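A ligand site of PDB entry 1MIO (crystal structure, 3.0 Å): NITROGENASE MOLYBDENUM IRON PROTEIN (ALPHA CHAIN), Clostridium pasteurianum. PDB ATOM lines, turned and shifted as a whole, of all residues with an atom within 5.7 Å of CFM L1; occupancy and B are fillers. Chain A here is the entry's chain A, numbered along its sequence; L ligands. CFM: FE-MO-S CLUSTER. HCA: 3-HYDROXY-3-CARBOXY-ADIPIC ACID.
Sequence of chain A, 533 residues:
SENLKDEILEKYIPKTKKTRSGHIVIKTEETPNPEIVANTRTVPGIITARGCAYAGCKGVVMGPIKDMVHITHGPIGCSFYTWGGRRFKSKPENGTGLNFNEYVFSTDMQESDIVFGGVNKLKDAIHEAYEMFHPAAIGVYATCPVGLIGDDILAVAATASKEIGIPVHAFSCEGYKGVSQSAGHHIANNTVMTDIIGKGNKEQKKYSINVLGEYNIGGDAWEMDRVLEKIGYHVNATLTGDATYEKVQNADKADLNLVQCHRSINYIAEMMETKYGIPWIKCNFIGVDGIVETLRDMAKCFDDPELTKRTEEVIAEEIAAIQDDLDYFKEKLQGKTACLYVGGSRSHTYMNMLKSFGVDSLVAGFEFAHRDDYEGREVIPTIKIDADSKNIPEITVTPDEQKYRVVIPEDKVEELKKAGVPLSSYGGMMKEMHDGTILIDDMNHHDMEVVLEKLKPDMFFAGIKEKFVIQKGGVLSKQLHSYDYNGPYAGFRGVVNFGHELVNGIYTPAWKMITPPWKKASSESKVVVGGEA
A ring nitrogen (ND1) of His 481 is bound to a molybdenum atom (MO1) of CFM L1, at 2.2 Å. SG of Cys 261 binds FE1 of CFM L1 (2.3 Å). The guanidinium group (NH1) of Arg 86 lies close to a sulfur (S5) of CFM L1 (2.7 Å). The backbone NH (N) of Gly 343 lies close to a sulfur (S3A) of CFM L1 (3.2 Å). A sulfur (S2B) of CFM L1 lies close to a ring nitrogen (NE2) of His 185, 3.2 Å away. N of Gly 344 lies close to S3A of CFM L1, 3.3 Å away. N of Arg 346 lies close to S3A of CFM L1, at 3.5 Å. A sulfur (S4B) of CFM L1 lies close to the guanidinium group (NH1) of Arg 346, at 3.4 Å. OG of Ser 264 lies close to S2A of CFM L1 (3.5 Å). NE2 of Gln 181 sits at hydrogen-bond distance from O2 of HCA L2 (2.8 Å).
A molybdenum atom (MO1) of CFM L1 is bound by an oxygen (O7) of HCA L2, 2.2 Å away.
The backbone carbonyl oxygen (O) of His 481 is in hydrogen-bond range of the guanidinium group (NH1) of Arg 346 (3.3 Å). SG of Cys 261 sits close to OG of Ser 264, 2.7 Å away. The side-chain sulfur (SG) of Cys 261 sits close to the backbone NH (N) of Arg 263 (3.5 Å). The backbone carbonyl oxygen (O) of Val 60 lies within hydrogen-bond range of the guanidinium group (NH2) of Arg 86. The side-chain hydroxyl (OG) of Ser 264 lies within hydrogen-bond range of the side-chain hydroxyl (OH) of Tyr 215. The guanidinium group (NH1) of Arg 346 sits at hydrogen-bond distance from the backbone carbonyl oxygen (O) of Leu 480. O of Val 342 sits at hydrogen-bond distance from N of Glu 367. The backbone NH (N) of Val 342 is in hydrogen-bond range of the side-chain hydroxyl (OG) of Ser 347.
Residues that only touch CFM L1: Tyr 215 (3.0 Å), Phe 368 (3.2 Å), Ile 217 (3.2 Å), Val 60 (3.6 Å), Val 342 (3.7 Å) and Ser 345 (3.9 Å). Of the 21 residues printed, 14 come within 4 Å of CFM L1. The nearest printed residue that does not touch CFM L1 is Gln 181 (4.2 Å).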
ATOM      1  N   GLY A  56      -6.100  33.416  20.982  1.00  0.00           N
ATOM      2  CA  GLY A  56      -5.786  32.430  21.982  1.00  0.00           C
ATOM      3  C   GLY A  56      -7.026  31.906  22.655  1.00  0.00           C
ATOM      4  O   GLY A  56      -7.042  30.733  22.996  1.00  0.00           O
ATOM      5  N   VAL A  60      -7.619  29.398  19.246  1.00  0.00           N
ATOM      6  CA  VAL A  60      -6.743  28.312  19.702  1.00  0.00           C
ATOM      7  C   VAL A  60      -7.378  27.278  20.596  1.00  0.00           C
ATOM      8  O   VAL A  60      -7.480  26.113  20.212  1.00  0.00           O
ATOM      9  CB  VAL A  60      -5.461  28.905  20.440  1.00  0.00           C
ATOM     10  CG1 VAL A  60      -4.641  27.808  21.125  1.00  0.00           C
ATOM     11  CG2 VAL A  60      -4.535  29.562  19.451  1.00  0.00           C
ATOM     12  N   ARG A  86      -6.162  27.506  11.281  1.00  0.00           N
ATOM     13  CA  ARG A  86      -5.586  26.738  12.396  1.00  0.00           C
ATOM     14  C   ARG A  86      -6.032  25.289  12.118  1.00  0.00           C
ATOM     15  O   ARG A  86      -7.229  25.000  12.077  1.00  0.00           O
ATOM     16  CB  ARG A  86      -6.132  27.265  13.752  1.00  0.00           C
ATOM     17  CG  ARG A  86      -5.159  27.604  14.906  1.00  0.00           C
ATOM     18  CD  ARG A  86      -4.342  26.469  15.509  1.00  0.00           C
ATOM     19  NE  ARG A  86      -5.134  25.773  16.509  1.00  0.00           N
ATOM     20  CZ  ARG A  86      -4.852  25.677  17.830  1.00  0.00           C
ATOM     21  NH1 ARG A  86      -3.771  26.214  18.381  1.00  0.00           N
ATOM     22  NH2 ARG A  86      -5.704  25.034  18.618  1.00  0.00           N
ATOM     23  N   GLN A 181      -1.426  36.153  22.605  1.00  0.00           N
ATOM     24  CA  GLN A 181      -2.379  35.059  22.682  1.00  0.00           C
ATOM     25  C   GLN A 181      -2.400  34.361  24.022  1.00  0.00           C
ATOM     26  O   GLN A 181      -3.303  33.552  24.204  1.00  0.00           O
ATOM     27  CB  GLN A 181      -2.119  33.970  21.666  1.00  0.00           C
ATOM     28  CG  GLN A 181      -2.237  34.309  20.200  1.00  0.00           C
ATOM     29  CD  GLN A 181      -0.885  34.606  19.585  1.00  0.00           C
ATOM     30  OE1 GLN A 181      -0.310  35.655  19.840  1.00  0.00           O
ATOM     31  NE2 GLN A 181      -0.300  33.710  18.804  1.00  0.00           N
ATOM     32  N   HIS A 185      -5.381  32.012  26.546  1.00  0.00           N
ATOM     33  CA  HIS A 185      -5.260  30.690  27.146  1.00  0.00           C
ATOM     34  C   HIS A 185      -5.558  30.759  28.633  1.00  0.00           C
ATOM     35  O   HIS A 185      -6.036  29.732  29.113  1.00  0.00           O
ATOM     36  CB  HIS A 185      -3.900  30.030  27.179  1.00  0.00           C
ATOM     37  CG  HIS A 185      -2.986  30.156  25.990  1.00  0.00           C
ATOM     38  ND1 HIS A 185      -1.706  30.491  25.900  1.00  0.00           N
ATOM     39  CD2 HIS A 185      -3.451  29.858  24.718  1.00  0.00           C
ATOM     40  CE1 HIS A 185      -1.393  30.411  24.633  1.00  0.00           C
ATOM     41  NE2 HIS A 185      -2.435  30.021  23.941  1.00  0.00           N
ATOM     42  N   TYR A 215      -4.522  19.916  20.503  1.00  0.00           N
ATOM     43  CA  TYR A 215      -5.587  20.447  19.668  1.00  0.00           C
ATOM     44  C   TYR A 215      -5.779  19.724  18.323  1.00  0.00           C
ATOM     45  O   TYR A 215      -6.602  20.108  17.500  1.00  0.00           O
ATOM     46  CB  TYR A 215      -5.249  21.954  19.488  1.00  0.00           C
ATOM     47  CG  TYR A 215      -4.931  22.653  20.815  1.00  0.00           C
ATOM     48  CD1 TYR A 215      -5.956  22.850  21.698  1.00  0.00           C
ATOM     49  CD2 TYR A 215      -3.626  23.007  21.177  1.00  0.00           C
ATOM     50  CE1 TYR A 215      -5.716  23.379  22.949  1.00  0.00           C
ATOM     51  CE2 TYR A 215      -3.365  23.547  22.435  1.00  0.00           C
ATOM     52  CZ  TYR A 215      -4.430  23.722  23.313  1.00  0.00           C
ATOM     53  OH  TYR A 215      -4.215  24.209  24.585  1.00  0.00           O
ATOM     54  N   ILE A 217      -3.512  19.011  15.454  1.00  0.00           N
ATOM     55  CA  ILE A 217      -3.154  19.646  14.198  1.00  0.00           C
ATOM     56  C   ILE A 217      -2.526  18.663  13.217  1.00  0.00           C
ATOM     57  O   ILE A 217      -1.463  18.038  13.372  1.00  0.00           O
ATOM     58  CB  ILE A 217      -2.247  20.863  14.536  1.00  0.00           C
ATOM     59  CG1 ILE A 217      -3.117  21.886  15.279  1.00  0.00           C
ATOM     60  CG2 ILE A 217      -1.581  21.463  13.298  1.00  0.00           C
ATOM     61  CD1 ILE A 217      -2.367  23.140  15.690  1.00  0.00           C
ATOM     62  N   CYS A 261       1.131  20.846  25.540  1.00  0.00           N
ATOM     63  CA  CYS A 261       1.540  22.236  25.609  1.00  0.00           C
ATOM     64  C   CYS A 261       1.438  22.773  27.037  1.00  0.00           C
ATOM     65  O   CYS A 261       0.384  22.870  27.708  1.00  0.00           O
ATOM     66  CB  CYS A 261       0.684  23.045  24.695  1.00  0.00           C
ATOM     67  SG  CYS A 261       1.042  24.806  24.785  1.00  0.00           S
ATOM     68  N   ARG A 263       2.261  26.029  27.858  1.00  0.00           N
ATOM     69  CA  ARG A 263       1.770  27.382  27.997  1.00  0.00           C
ATOM     70  C   ARG A 263       0.259  27.457  27.961  1.00  0.00           C
ATOM     71  O   ARG A 263      -0.318  28.250  28.696  1.00  0.00           O
ATOM     72  CB  ARG A 263       2.290  28.291  26.911  1.00  0.00           C
ATOM     73  CG  ARG A 263       1.909  29.732  27.139  1.00  0.00           C
ATOM     74  CD  ARG A 263       2.667  30.274  28.309  1.00  0.00           C
ATOM     75  NE  ARG A 263       1.821  30.569  29.445  1.00  0.00           N
ATOM     76  CZ  ARG A 263       2.045  30.099  30.679  1.00  0.00           C
ATOM     77  NH1 ARG A 263       3.054  29.315  31.007  1.00  0.00           N
ATOM     78  NH2 ARG A 263       1.213  30.460  31.633  1.00  0.00           N
ATOM     79  N   SER A 264      -0.386  26.654  27.150  1.00  0.00           N
ATOM     80  CA  SER A 264      -1.806  26.750  27.063  1.00  0.00           C
ATOM     81  C   SER A 264      -2.524  26.096  28.195  1.00  0.00           C
ATOM     82  O   SER A 264      -3.081  26.876  28.957  1.00  0.00           O
ATOM     83  CB  SER A 264      -2.279  26.170  25.792  1.00  0.00           C
ATOM     84  OG  SER A 264      -1.533  24.990  25.534  1.00  0.00           O
ATOM     85  N   VAL A 342       8.687  30.025  17.457  1.00  0.00           N
ATOM     86  CA  VAL A 342       7.336  29.506  17.267  1.00  0.00           C
ATOM     87  C   VAL A 342       6.482  30.163  18.357  1.00  0.00           C
ATOM     88  O   VAL A 342       6.816  31.229  18.857  1.00  0.00           O
ATOM     89  CB  VAL A 342       7.332  27.940  17.359  1.00  0.00           C
ATOM     90  CG1 VAL A 342       6.152  27.434  16.590  1.00  0.00           C
ATOM     91  CG2 VAL A 342       8.473  27.265  16.613  1.00  0.00           C
ATOM     92  N   GLY A 343       5.335  29.634  18.724  1.00  0.00           N
ATOM     93  CA  GLY A 343       4.447  30.249  19.696  1.00  0.00           C
ATOM     94  C   GLY A 343       4.903  30.116  21.123  1.00  0.00           C
ATOM     95  O   GLY A 343       5.593  31.015  21.580  1.00  0.00           O
ATOM     96  N   GLY A 344       4.567  29.069  21.886  1.00  0.00           N
ATOM     97  CA  GLY A 344       5.019  28.973  23.286  1.00  0.00           C
ATOM     98  C   GLY A 344       5.232  27.577  23.860  1.00  0.00           C
ATOM     99  O   GLY A 344       4.967  27.319  25.027  1.00  0.00           O
ATOM    100  N   SER A 345       5.770  26.696  23.026  1.00  0.00           N
ATOM    101  CA  SER A 345       5.975  25.289  23.298  1.00  0.00           C
ATOM    102  C   SER A 345       6.764  24.682  22.127  1.00  0.00           C
ATOM    103  O   SER A 345       7.860  24.183  22.334  1.00  0.00           O
ATOM    104  CB  SER A 345       4.595  24.617  23.489  1.00  0.00           C
ATOM    105  OG  SER A 345       4.452  23.221  23.212  1.00  0.00           O
ATOM    106  N   ARG A 346       6.339  24.767  20.865  1.00  0.00           N
ATOM    107  CA  ARG A 346       7.026  24.099  19.767  1.00  0.00           C
ATOM    108  C   ARG A 346       8.490  24.329  19.527  1.00  0.00           C
ATOM    109  O   ARG A 346       9.183  23.350  19.234  1.00  0.00           O
ATOM    110  CB  ARG A 346       6.296  24.373  18.473  1.00  0.00           C
ATOM    111  CG  ARG A 346       5.083  23.543  18.696  1.00  0.00           C
ATOM    112  CD  ARG A 346       4.127  23.422  17.569  1.00  0.00           C
ATOM    113  NE  ARG A 346       2.978  22.683  18.039  1.00  0.00           N
ATOM    114  CZ  ARG A 346       1.878  22.545  17.294  1.00  0.00           C
ATOM    115  NH1 ARG A 346       1.767  23.072  16.067  1.00  0.00           N
ATOM    116  NH2 ARG A 346       0.832  21.909  17.825  1.00  0.00           N
ATOM    117  N   SER A 347       9.014  25.553  19.716  1.00  0.00           N
ATOM    118  CA  SER A 347      10.451  25.829  19.562  1.00  0.00           C
ATOM    119  C   SER A 347      11.294  24.932  20.464  1.00  0.00           C
ATOM    120  O   SER A 347      12.457  24.654  20.245  1.00  0.00           O
ATOM    121  CB  SER A 347      10.748  27.272  19.920  1.00  0.00           C
ATOM    122  OG  SER A 347       9.605  28.066  19.702  1.00  0.00           O
ATOM    123  N   GLU A 367       7.147  33.506  20.697  1.00  0.00           N
ATOM    124  CA  GLU A 367       6.265  34.619  20.465  1.00  0.00           C
ATOM    125  C   GLU A 367       5.751  35.243  21.771  1.00  0.00           C
ATOM    126  O   GLU A 367       6.134  36.331  22.175  1.00  0.00           O
ATOM    127  CB  GLU A 367       5.152  34.039  19.594  1.00  0.00           C
ATOM    128  CG  GLU A 367       4.414  34.986  18.690  1.00  0.00           C
ATOM    129  CD  GLU A 367       4.055  34.292  17.389  1.00  0.00           C
ATOM    130  OE1 GLU A 367       4.965  33.904  16.655  1.00  0.00           O
ATOM    131  OE2 GLU A 367       2.869  34.128  17.119  1.00  0.00           O
ATOM    132  N   PHE A 368       4.940  34.509  22.509  1.00  0.00           N
ATOM    133  CA  PHE A 368       4.255  35.000  23.681  1.00  0.00           C
ATOM    134  C   PHE A 368       4.576  34.166  24.918  1.00  0.00           C
ATOM    135  O   PHE A 368       3.864  34.330  25.929  1.00  0.00           O
ATOM    136  CB  PHE A 368       2.730  34.977  23.432  1.00  0.00           C
ATOM    137  CG  PHE A 368       2.186  33.602  23.069  1.00  0.00           C
ATOM    138  CD1 PHE A 368       2.084  32.589  24.013  1.00  0.00           C
ATOM    139  CD2 PHE A 368       1.935  33.292  21.748  1.00  0.00           C
ATOM    140  CE1 PHE A 368       1.762  31.307  23.664  1.00  0.00           C
ATOM    141  CE2 PHE A 368       1.621  31.982  21.407  1.00  0.00           C
ATOM    142  CZ  PHE A 368       1.536  30.994  22.360  1.00  0.00           C
ATOM    143  N   LEU A 480       6.173  25.298  11.517  1.00  0.00           N
ATOM    144  CA  LEU A 480       6.008  24.571  12.763  1.00  0.00           C
ATOM    145  C   LEU A 480       4.666  24.667  13.464  1.00  0.00           C
ATOM    146  O   LEU A 480       4.377  23.909  14.372  1.00  0.00           O
ATOM    147  CB  LEU A 480       7.135  25.022  13.658  1.00  0.00           C
ATOM    148  CG  LEU A 480       7.898  23.875  14.268  1.00  0.00           C
ATOM    149  CD1 LEU A 480       8.125  22.782  13.216  1.00  0.00           C
ATOM    150  CD2 LEU A 480       9.173  24.431  14.895  1.00  0.00           C
ATOM    151  N   HIS A 481       3.874  25.638  13.022  1.00  0.00           N
ATOM    152  CA  HIS A 481       2.506  25.834  13.447  1.00  0.00           C
ATOM    153  C   HIS A 481       1.603  24.971  12.567  1.00  0.00           C
ATOM    154  O   HIS A 481       1.018  23.989  13.023  1.00  0.00           O
ATOM    155  CB  HIS A 481       2.101  27.283  13.265  1.00  0.00           C
ATOM    156  CG  HIS A 481       2.626  28.318  14.253  1.00  0.00           C
ATOM    157  ND1 HIS A 481       1.886  29.089  15.039  1.00  0.00           N
ATOM    158  CD2 HIS A 481       3.879  28.880  14.257  1.00  0.00           C
ATOM    159  CE1 HIS A 481       2.632  30.072  15.501  1.00  0.00           C
ATOM    160  NE2 HIS A 481       3.826  29.939  15.021  1.00  0.00           N
ATOM    161  N   SER A 482       1.509  25.303  11.280  1.00  0.00           N
ATOM    162  CA  SER A 482       0.685  24.621  10.284  1.00  0.00           C
ATOM    163  C   SER A 482       1.226  23.321   9.707  1.00  0.00           C
ATOM    164  O   SER A 482       0.579  22.754   8.803  1.00  0.00           O
ATOM    165  CB  SER A 482       0.441  25.489   9.078  1.00  0.00           C
ATOM    166  OG  SER A 482       1.601  25.495   8.255  1.00  0.00           O
HETATM  167 FE1  CFM L   1       0.507  25.764  22.753  1.00  0.00          FE
HETATM  168 FE2  CFM L   1      -0.423  27.852  21.475  1.00  0.00          FE
HETATM  169 FE3  CFM L   1      -0.537  25.312  20.342  1.00  0.00          FE
HETATM  170 FE4  CFM L   1       2.131  26.533  20.806  1.00  0.00          FE
HETATM  171 FE5  CFM L   1       1.944  27.534  18.486  1.00  0.00          FE
HETATM  172 FE6  CFM L   1      -0.408  28.979  19.062  1.00  0.00          FE
HETATM  173 FE7  CFM L   1      -0.610  26.423  18.123  1.00  0.00          FE
HETATM  174 MO1  CFM L   1       0.330  28.525  16.481  1.00  0.00          MO
HETATM  175  S1A CFM L   1       1.566  27.793  22.607  1.00  0.00           S
HETATM  176  S4A CFM L   1       1.374  24.349  21.127  1.00  0.00           S
HETATM  177  S3A CFM L   1       3.921  26.875  19.476  1.00  0.00           S
HETATM  178  S2A CFM L   1      -1.693  26.077  22.195  1.00  0.00           S
HETATM  179  S1B CFM L   1       1.475  29.784  18.121  1.00  0.00           S
HETATM  180  S2B CFM L   1      -1.290  29.899  20.913  1.00  0.00           S
HETATM  181  S3B CFM L   1      -1.799  28.279  17.416  1.00  0.00           S
HETATM  182  S4B CFM L   1       1.165  26.350  16.698  1.00  0.00           S
HETATM  183  S5  CFM L   1      -1.724  24.517  18.544  1.00  0.00           S
HETATM  184  C1  HCA L   2      -2.641  32.150  15.971  1.00  0.00           C
HETATM  185  C2  HCA L   2      -2.417  31.428  14.641  1.00  0.00           C
HETATM  186  C3  HCA L   2      -1.194  30.492  14.520  1.00  0.00           C
HETATM  187  C4  HCA L   2      -0.230  31.206  13.529  1.00  0.00           C
HETATM  188  C5  HCA L   2      -0.031  30.702  12.109  1.00  0.00           C
HETATM  189  C6  HCA L   2       1.393  30.654  11.571  1.00  0.00           C
HETATM  190  C7  HCA L   2      -1.613  29.079  14.109  1.00  0.00           C
HETATM  191  O1  HCA L   2      -3.816  32.201  16.536  1.00  0.00           O
HETATM  192  O2  HCA L   2      -1.701  32.863  16.498  1.00  0.00           O
HETATM  193  O3  HCA L   2       2.085  31.764  11.469  1.00  0.00           O
HETATM  194  O4  HCA L   2       1.795  29.598  10.921  1.00  0.00           O
HETATM  195  O5  HCA L   2      -1.088  27.991  14.885  1.00  0.00           O
HETATM  196  O6  HCA L   2      -2.404  28.873  13.218  1.00  0.00           O
HETATM  197  O7  HCA L   2      -0.548  30.405  15.793  1.00  0.00           O
